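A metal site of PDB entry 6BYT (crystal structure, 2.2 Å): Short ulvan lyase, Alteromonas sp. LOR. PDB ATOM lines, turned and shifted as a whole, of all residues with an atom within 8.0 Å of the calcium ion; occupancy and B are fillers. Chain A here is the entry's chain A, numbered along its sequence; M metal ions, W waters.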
ATOM      1  N   VAL A 159      18.045 -13.989 -11.809  1.00  0.00           N
ATOM      2  CA  VAL A 159      18.946 -14.546 -12.795  1.00  0.00           C
ATOM      3  C   VAL A 159      19.650 -15.766 -12.224  1.00  0.00           C
ATOM      4  O   VAL A 159      20.195 -15.735 -11.116  1.00  0.00           O
ATOM      5  CB  VAL A 159      19.946 -13.477 -13.240  1.00  0.00           C
ATOM      6  CG1 VAL A 159      21.028 -14.097 -14.070  1.00  0.00           C
ATOM      7  CG2 VAL A 159      19.199 -12.384 -13.992  1.00  0.00           C
ATOM      8  N   ASP A 160      19.638 -16.866 -12.980  1.00  0.00           N
ATOM      9  CA  ASP A 160      20.210 -18.135 -12.520  1.00  0.00           C
ATOM     10  C   ASP A 160      19.558 -18.645 -11.242  1.00  0.00           C
ATOM     11  O   ASP A 160      20.186 -19.415 -10.496  1.00  0.00           O
ATOM     12  CB  ASP A 160      21.727 -18.033 -12.315  1.00  0.00           C
ATOM     13  CG  ASP A 160      22.444 -17.452 -13.507  1.00  0.00           C
ATOM     14  OD1 ASP A 160      21.920 -17.593 -14.623  1.00  0.00           O
ATOM     15  OD2 ASP A 160      23.546 -16.896 -13.332  1.00  0.00           O
ATOM     16  N   ASP A 161      18.311 -18.249 -10.954  1.00  0.00           N
ATOM     17  CA  ASP A 161      17.673 -18.638  -9.690  1.00  0.00           C
ATOM     18  C   ASP A 161      16.148 -18.554  -9.771  1.00  0.00           C
ATOM     19  O   ASP A 161      15.474 -18.332  -8.753  1.00  0.00           O
ATOM     20  CB  ASP A 161      18.224 -17.755  -8.558  1.00  0.00           C
ATOM     21  CG  ASP A 161      17.946 -18.308  -7.154  1.00  0.00           C
ATOM     22  OD1 ASP A 161      18.015 -19.544  -6.954  1.00  0.00           O
ATOM     23  OD2 ASP A 161      17.699 -17.491  -6.241  1.00  0.00           O
ATOM     24  N   PHE A 162      15.585 -18.761 -10.953  1.00  0.00           N
ATOM     25  CA  PHE A 162      14.149 -18.606 -11.151  1.00  0.00           C
ATOM     26  C   PHE A 162      13.366 -19.866 -10.872  1.00  0.00           C
ATOM     27  O   PHE A 162      12.143 -19.819 -10.790  1.00  0.00           O
ATOM     28  CB  PHE A 162      13.848 -18.136 -12.580  1.00  0.00           C
ATOM     29  CG  PHE A 162      14.562 -18.932 -13.645  1.00  0.00           C
ATOM     30  CD1 PHE A 162      14.080 -20.176 -14.049  1.00  0.00           C
ATOM     31  CD2 PHE A 162      15.698 -18.419 -14.263  1.00  0.00           C
ATOM     32  CE1 PHE A 162      14.740 -20.902 -15.055  1.00  0.00           C
ATOM     33  CE2 PHE A 162      16.350 -19.127 -15.283  1.00  0.00           C
ATOM     34  CZ  PHE A 162      15.884 -20.380 -15.665  1.00  0.00           C
ATOM     35  N   PHE A 163      14.064 -20.998 -10.758  1.00  0.00           N
ATOM     36  CA  PHE A 163      13.522 -22.263 -10.295  1.00  0.00           C
ATOM     37  C   PHE A 163      14.428 -22.741  -9.169  1.00  0.00           C
ATOM     38  O   PHE A 163      15.647 -22.851  -9.368  1.00  0.00           O
ATOM     39  CB  PHE A 163      13.494 -23.288 -11.432  1.00  0.00           C
ATOM     40  CG  PHE A 163      12.716 -24.530 -11.103  1.00  0.00           C
ATOM     41  CD1 PHE A 163      13.341 -25.615 -10.472  1.00  0.00           C
ATOM     42  CD2 PHE A 163      11.361 -24.628 -11.442  1.00  0.00           C
ATOM     43  CE1 PHE A 163      12.619 -26.784 -10.180  1.00  0.00           C
ATOM     44  CE2 PHE A 163      10.622 -25.793 -11.163  1.00  0.00           C
ATOM     45  CZ  PHE A 163      11.262 -26.874 -10.513  1.00  0.00           C
ATOM     46  N   ARG A 164      13.831 -23.016  -8.015  1.00  0.00           N
ATOM     47  CA  ARG A 164      14.577 -23.239  -6.764  1.00  0.00           C
ATOM     48  C   ARG A 164      14.273 -24.655  -6.252  1.00  0.00           C
ATOM     49  O   ARG A 164      13.228 -24.891  -5.635  1.00  0.00           O
ATOM     50  CB  ARG A 164      14.211 -22.172  -5.721  1.00  0.00           C
ATOM     51  CG  ARG A 164      14.685 -20.765  -6.092  1.00  0.00           C
ATOM     52  CD  ARG A 164      13.924 -19.607  -5.417  1.00  0.00           C
ATOM     53  NE  ARG A 164      14.595 -18.359  -5.741  1.00  0.00           N
ATOM     54  CZ  ARG A 164      14.249 -17.156  -5.301  1.00  0.00           C
ATOM     55  NH1 ARG A 164      13.203 -16.990  -4.500  1.00  0.00           N
ATOM     56  NH2 ARG A 164      14.975 -16.107  -5.649  1.00  0.00           N
ATOM     57  N   TYR A 165      15.209 -25.577  -6.496  1.00  0.00           N
ATOM     58  CA  TYR A 165      15.064 -26.982  -6.150  1.00  0.00           C
ATOM     59  C   TYR A 165      16.195 -27.403  -5.218  1.00  0.00           C
ATOM     60  O   TYR A 165      17.378 -27.184  -5.534  1.00  0.00           O
ATOM     61  CB  TYR A 165      15.101 -27.832  -7.425  1.00  0.00           C
ATOM     62  CG  TYR A 165      15.107 -29.330  -7.256  1.00  0.00           C
ATOM     63  CD1 TYR A 165      14.222 -29.963  -6.419  1.00  0.00           C
ATOM     64  CD2 TYR A 165      16.006 -30.125  -7.974  1.00  0.00           C
ATOM     65  CE1 TYR A 165      14.226 -31.331  -6.285  1.00  0.00           C
ATOM     66  CE2 TYR A 165      16.022 -31.501  -7.843  1.00  0.00           C
ATOM     67  CZ  TYR A 165      15.132 -32.104  -6.998  1.00  0.00           C
ATOM     68  OH  TYR A 165      15.135 -33.477  -6.856  1.00  0.00           O
ATOM     69  N   LYS A 187      24.721 -29.548  -2.956  1.00  0.00           N
ATOM     70  CA  LYS A 187      24.985 -28.150  -3.280  1.00  0.00           C
ATOM     71  C   LYS A 187      24.903 -27.939  -4.785  1.00  0.00           C
ATOM     72  O   LYS A 187      25.093 -28.859  -5.572  1.00  0.00           O
ATOM     73  CB  LYS A 187      26.372 -27.725  -2.776  1.00  0.00           C
ATOM     74  CG  LYS A 187      26.487 -27.444  -1.275  1.00  0.00           C
ATOM     75  CD  LYS A 187      27.802 -26.788  -0.962  1.00  0.00           C
ATOM     76  CE  LYS A 187      27.931 -26.462   0.511  1.00  0.00           C
ATOM     77  NZ  LYS A 187      29.350 -26.103   0.843  1.00  0.00           N
ATOM     78  N   ASP A 188      24.603 -26.697  -5.167  1.00  0.00           N
ATOM     79  CA  ASP A 188      24.743 -26.268  -6.563  1.00  0.00           C
ATOM     80  C   ASP A 188      26.224 -26.039  -6.832  1.00  0.00           C
ATOM     81  O   ASP A 188      26.817 -25.082  -6.327  1.00  0.00           O
ATOM     82  CB  ASP A 188      23.912 -25.013  -6.795  1.00  0.00           C
ATOM     83  CG  ASP A 188      23.901 -24.545  -8.258  1.00  0.00           C
ATOM     84  OD1 ASP A 188      24.693 -25.056  -9.091  1.00  0.00           O
ATOM     85  OD2 ASP A 188      23.108 -23.631  -8.564  1.00  0.00           O
ATOM     86  N   THR A 189      26.836 -26.914  -7.617  1.00  0.00           N
ATOM     87  CA  THR A 189      28.230 -26.769  -7.999  1.00  0.00           C
ATOM     88  C   THR A 189      28.361 -26.701  -9.517  1.00  0.00           C
ATOM     89  O   THR A 189      29.287 -27.257 -10.105  1.00  0.00           O
ATOM     90  CB  THR A 189      29.090 -27.911  -7.452  1.00  0.00           C
ATOM     91  OG1 THR A 189      28.778 -29.127  -8.143  1.00  0.00           O
ATOM     92  CG2 THR A 189      28.858 -28.094  -5.947  1.00  0.00           C
ATOM     93  N   SER A 190      27.422 -26.018 -10.170  1.00  0.00           N
ATOM     94  CA  SER A 190      27.447 -25.914 -11.613  1.00  0.00           C
ATOM     95  C   SER A 190      28.109 -24.608 -12.035  1.00  0.00           C
ATOM     96  O   SER A 190      28.552 -23.807 -11.203  1.00  0.00           O
ATOM     97  CB  SER A 190      26.030 -26.020 -12.179  1.00  0.00           C
ATOM     98  OG  SER A 190      25.265 -24.881 -11.825  1.00  0.00           O
ATOM     99  N   LEU A 192      26.682 -22.088 -12.943  1.00  0.00           N
ATOM    100  CA  LEU A 192      25.849 -20.986 -12.481  1.00  0.00           C
ATOM    101  C   LEU A 192      25.774 -20.858 -10.966  1.00  0.00           C
ATOM    102  O   LEU A 192      25.077 -19.978 -10.477  1.00  0.00           O
ATOM    103  CB  LEU A 192      24.436 -21.109 -13.057  1.00  0.00           C
ATOM    104  CG  LEU A 192      24.396 -21.165 -14.598  1.00  0.00           C
ATOM    105  CD1 LEU A 192      22.967 -21.221 -15.133  1.00  0.00           C
ATOM    106  CD2 LEU A 192      25.140 -19.963 -15.207  1.00  0.00           C
ATOM    107  N   SER A 193      26.461 -21.727 -10.211  1.00  0.00           N
ATOM    108  CA  SER A 193      26.418 -21.682  -8.745  1.00  0.00           C
ATOM    109  C   SER A 193      26.699 -20.287  -8.222  1.00  0.00           C
ATOM    110  O   SER A 193      27.696 -19.658  -8.597  1.00  0.00           O
ATOM    111  CB  SER A 193      27.434 -22.654  -8.135  1.00  0.00           C
ATOM    112  OG  SER A 193      27.363 -22.654  -6.705  1.00  0.00           O
ATOM    113  N   GLN A 194      25.846 -19.817  -7.308  1.00  0.00           N
ATOM    114  CA  GLN A 194      26.084 -18.495  -6.722  1.00  0.00           C
ATOM    115  C   GLN A 194      27.055 -18.541  -5.547  1.00  0.00           C
ATOM    116  O   GLN A 194      27.354 -17.472  -4.995  1.00  0.00           O
ATOM    117  CB  GLN A 194      24.763 -17.856  -6.274  1.00  0.00           C
ATOM    118  CG  GLN A 194      23.694 -17.746  -7.378  1.00  0.00           C
ATOM    119  CD  GLN A 194      22.354 -17.195  -6.835  1.00  0.00           C
ATOM    120  OE1 GLN A 194      21.673 -17.864  -6.050  1.00  0.00           O
ATOM    121  NE2 GLN A 194      21.962 -16.006  -7.285  1.00  0.00           N
ATOM    122  N   GLY A 195      27.544 -19.704  -5.120  1.00  0.00           N
ATOM    123  CA  GLY A 195      28.594 -19.756  -4.117  1.00  0.00           C
ATOM    124  C   GLY A 195      28.457 -20.974  -3.214  1.00  0.00           C
ATOM    125  O   GLY A 195      27.682 -21.878  -3.490  1.00  0.00           O
ATOM    126  N   ASP A 197      27.165 -21.449  -0.191  1.00  0.00           N
ATOM    127  CA  ASP A 197      25.907 -21.782   0.474  1.00  0.00           C
ATOM    128  C   ASP A 197      24.776 -21.869  -0.531  1.00  0.00           C
ATOM    129  O   ASP A 197      23.611 -21.599  -0.200  1.00  0.00           O
ATOM    130  CB  ASP A 197      25.583 -20.761   1.568  1.00  0.00           C
ATOM    131  CG  ASP A 197      25.496 -19.350   1.040  1.00  0.00           C
ATOM    132  OD1 ASP A 197      25.521 -19.180  -0.199  1.00  0.00           O
ATOM    133  OD2 ASP A 197      25.435 -18.408   1.845  1.00  0.00           O
ATOM    134  N   ASP A 198      25.105 -22.193  -1.780  1.00  0.00           N
ATOM    135  CA  ASP A 198      24.110 -22.354  -2.842  1.00  0.00           C
ATOM    136  C   ASP A 198      23.591 -23.795  -2.786  1.00  0.00           C
ATOM    137  O   ASP A 198      24.281 -24.725  -3.236  1.00  0.00           O
ATOM    138  CB  ASP A 198      24.724 -22.013  -4.193  1.00  0.00           C
ATOM    139  CG  ASP A 198      23.660 -21.858  -5.290  1.00  0.00           C
ATOM    140  OD1 ASP A 198      22.493 -22.253  -5.051  1.00  0.00           O
ATOM    141  OD2 ASP A 198      24.017 -21.361  -6.396  1.00  0.00           O
ATOM    142  N   TYR A 199      22.392 -23.970  -2.235  1.00  0.00           N
ATOM    143  CA  TYR A 199      21.682 -25.257  -2.215  1.00  0.00           C
ATOM    144  C   TYR A 199      20.525 -25.307  -3.213  1.00  0.00           C
ATOM    145  O   TYR A 199      19.780 -26.291  -3.230  1.00  0.00           O
ATOM    146  CB  TYR A 199      21.155 -25.576  -0.806  1.00  0.00           C
ATOM    147  CG  TYR A 199      22.230 -26.098   0.132  1.00  0.00           C
ATOM    148  CD1 TYR A 199      23.053 -25.227   0.849  1.00  0.00           C
ATOM    149  CD2 TYR A 199      22.456 -27.464   0.254  1.00  0.00           C
ATOM    150  CE1 TYR A 199      24.058 -25.721   1.693  1.00  0.00           C
ATOM    151  CE2 TYR A 199      23.435 -27.955   1.082  1.00  0.00           C
ATOM    152  CZ  TYR A 199      24.246 -27.090   1.805  1.00  0.00           C
ATOM    153  OH  TYR A 199      25.231 -27.606   2.617  1.00  0.00           O
ATOM    154  N   LYS A 200      20.378 -24.290  -4.044  1.00  0.00           N
ATOM    155  CA  LYS A 200      19.252 -24.180  -4.976  1.00  0.00           C
ATOM    156  C   LYS A 200      19.691 -24.591  -6.369  1.00  0.00           C
ATOM    157  O   LYS A 200      20.669 -24.057  -6.910  1.00  0.00           O
ATOM    158  CB  LYS A 200      18.711 -22.742  -4.996  1.00  0.00           C
ATOM    159  CG  LYS A 200      18.086 -22.297  -3.694  1.00  0.00           C
ATOM    160  CD  LYS A 200      17.694 -20.818  -3.777  1.00  0.00           C
ATOM    161  CE  LYS A 200      18.904 -19.921  -3.643  1.00  0.00           C
ATOM    162  NZ  LYS A 200      18.562 -18.477  -3.824  1.00  0.00           N
ATOM    163  N   HIS A 201      18.975 -25.554  -6.954  1.00  0.00           N
ATOM    164  CA  HIS A 201      19.259 -26.036  -8.295  1.00  0.00           C
ATOM    165  C   HIS A 201      18.283 -25.421  -9.283  1.00  0.00           C
ATOM    166  O   HIS A 201      17.112 -25.201  -8.951  1.00  0.00           O
ATOM    167  CB  HIS A 201      19.190 -27.567  -8.336  1.00  0.00           C
ATOM    168  CG  HIS A 201      20.251 -28.199  -7.500  1.00  0.00           C
ATOM    169  ND1 HIS A 201      21.481 -28.563  -8.002  1.00  0.00           N
ATOM    170  CD2 HIS A 201      20.292 -28.457  -6.170  1.00  0.00           C
ATOM    171  CE1 HIS A 201      22.231 -29.049  -7.025  1.00  0.00           C
ATOM    172  NE2 HIS A 201      21.534 -29.001  -5.908  1.00  0.00           N
ATOM    173  N   LEU A 202      18.773 -25.099 -10.478  1.00  0.00           N
ATOM    174  CA  LEU A 202      17.953 -24.405 -11.452  1.00  0.00           C
ATOM    175  C   LEU A 202      17.082 -25.344 -12.275  1.00  0.00           C
ATOM    176  O   LEU A 202      16.091 -24.886 -12.859  1.00  0.00           O
ATOM    177  CB  LEU A 202      18.822 -23.558 -12.370  1.00  0.00           C
ATOM    178  CG  LEU A 202      18.073 -22.515 -13.217  1.00  0.00           C
ATOM    179  CD1 LEU A 202      17.213 -21.591 -12.379  1.00  0.00           C
ATOM    180  CD2 LEU A 202      19.049 -21.728 -14.091  1.00  0.00           C
ATOM    181  N   THR A 203      17.429 -26.627 -12.353  1.00  0.00           N
ATOM    182  CA  THR A 203      16.628 -27.640 -13.027  1.00  0.00           C
ATOM    183  C   THR A 203      16.561 -28.875 -12.145  1.00  0.00           C
ATOM    184  O   THR A 203      17.353 -29.019 -11.198  1.00  0.00           O
ATOM    185  CB  THR A 203      17.186 -28.044 -14.402  1.00  0.00           C
ATOM    186  OG1 THR A 203      18.292 -28.935 -14.219  1.00  0.00           O
ATOM    187  CG2 THR A 203      17.613 -26.825 -15.227  1.00  0.00           C
ATOM    188  N   LEU A 208      21.670 -28.102 -17.256  1.00  0.00           N
ATOM    189  CA  LEU A 208      21.341 -26.677 -17.362  1.00  0.00           C
ATOM    190  C   LEU A 208      20.782 -26.296 -18.734  1.00  0.00           C
ATOM    191  O   LEU A 208      20.104 -25.266 -18.851  1.00  0.00           O
ATOM    192  CB  LEU A 208      22.563 -25.810 -17.037  1.00  0.00           C
ATOM    193  CG  LEU A 208      22.935 -25.653 -15.563  1.00  0.00           C
ATOM    194  CD1 LEU A 208      24.214 -24.833 -15.392  1.00  0.00           C
ATOM    195  CD2 LEU A 208      21.802 -25.036 -14.808  1.00  0.00           C
HETATM  196 CA    CA M   1      21.784 -22.092  -7.512  1.00  0.00          CA
HETATM  197  O   HOH W   1      22.529 -20.328  -9.127  1.00  0.00           O
HETATM  198  O   HOH W   2      20.083 -22.042  -9.322  1.00  0.00           O
HETATM  199  O   HOH W   3      20.812 -20.052  -6.756  1.00  0.00           O
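The backbone carbonyl oxygen of Asp 188 sits at hydrogen-bond distance from the side-chain hydroxyl of Ser 193, 2.5 Å away.
The side-chain hydroxyl (OG) of Ser 190 lies within hydrogen-bond range of the side-chain carboxylate (OD1) of Asp 188, at 2.8 Å.
OD2 of Asp 161 lies within salt-bridge range of NZ of Lys 200 (2.7 Å).
N of Gln 194 lies close to OD2 of Asp 198.
Three residues have an atom within 4 Å of the calcium ion: Asp 188, Asp 198 and Lys 200.
Water W3 bridges OE1 of Gln 194 (2.5 Å) and OD1 of Asp 161 (2.8 Å).
Water W1 bridges the backbone carbonyl oxygen of Asp 160 (2.9 Å) and the backbone carbonyl oxygen of Leu 192 (2.9 Å).
The calcium ion is bound by the side-chain carboxylate (OD2) of Asp 188, the backbone carbonyl oxygen (O) of Lys 200, water W3, water W2, water W1, the side-chain carboxylate (OD1) of Asp 198 and the side-chain carboxylate (OD2) of Asp 198.
The calcium ion has seven donor atoms within binding distance.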
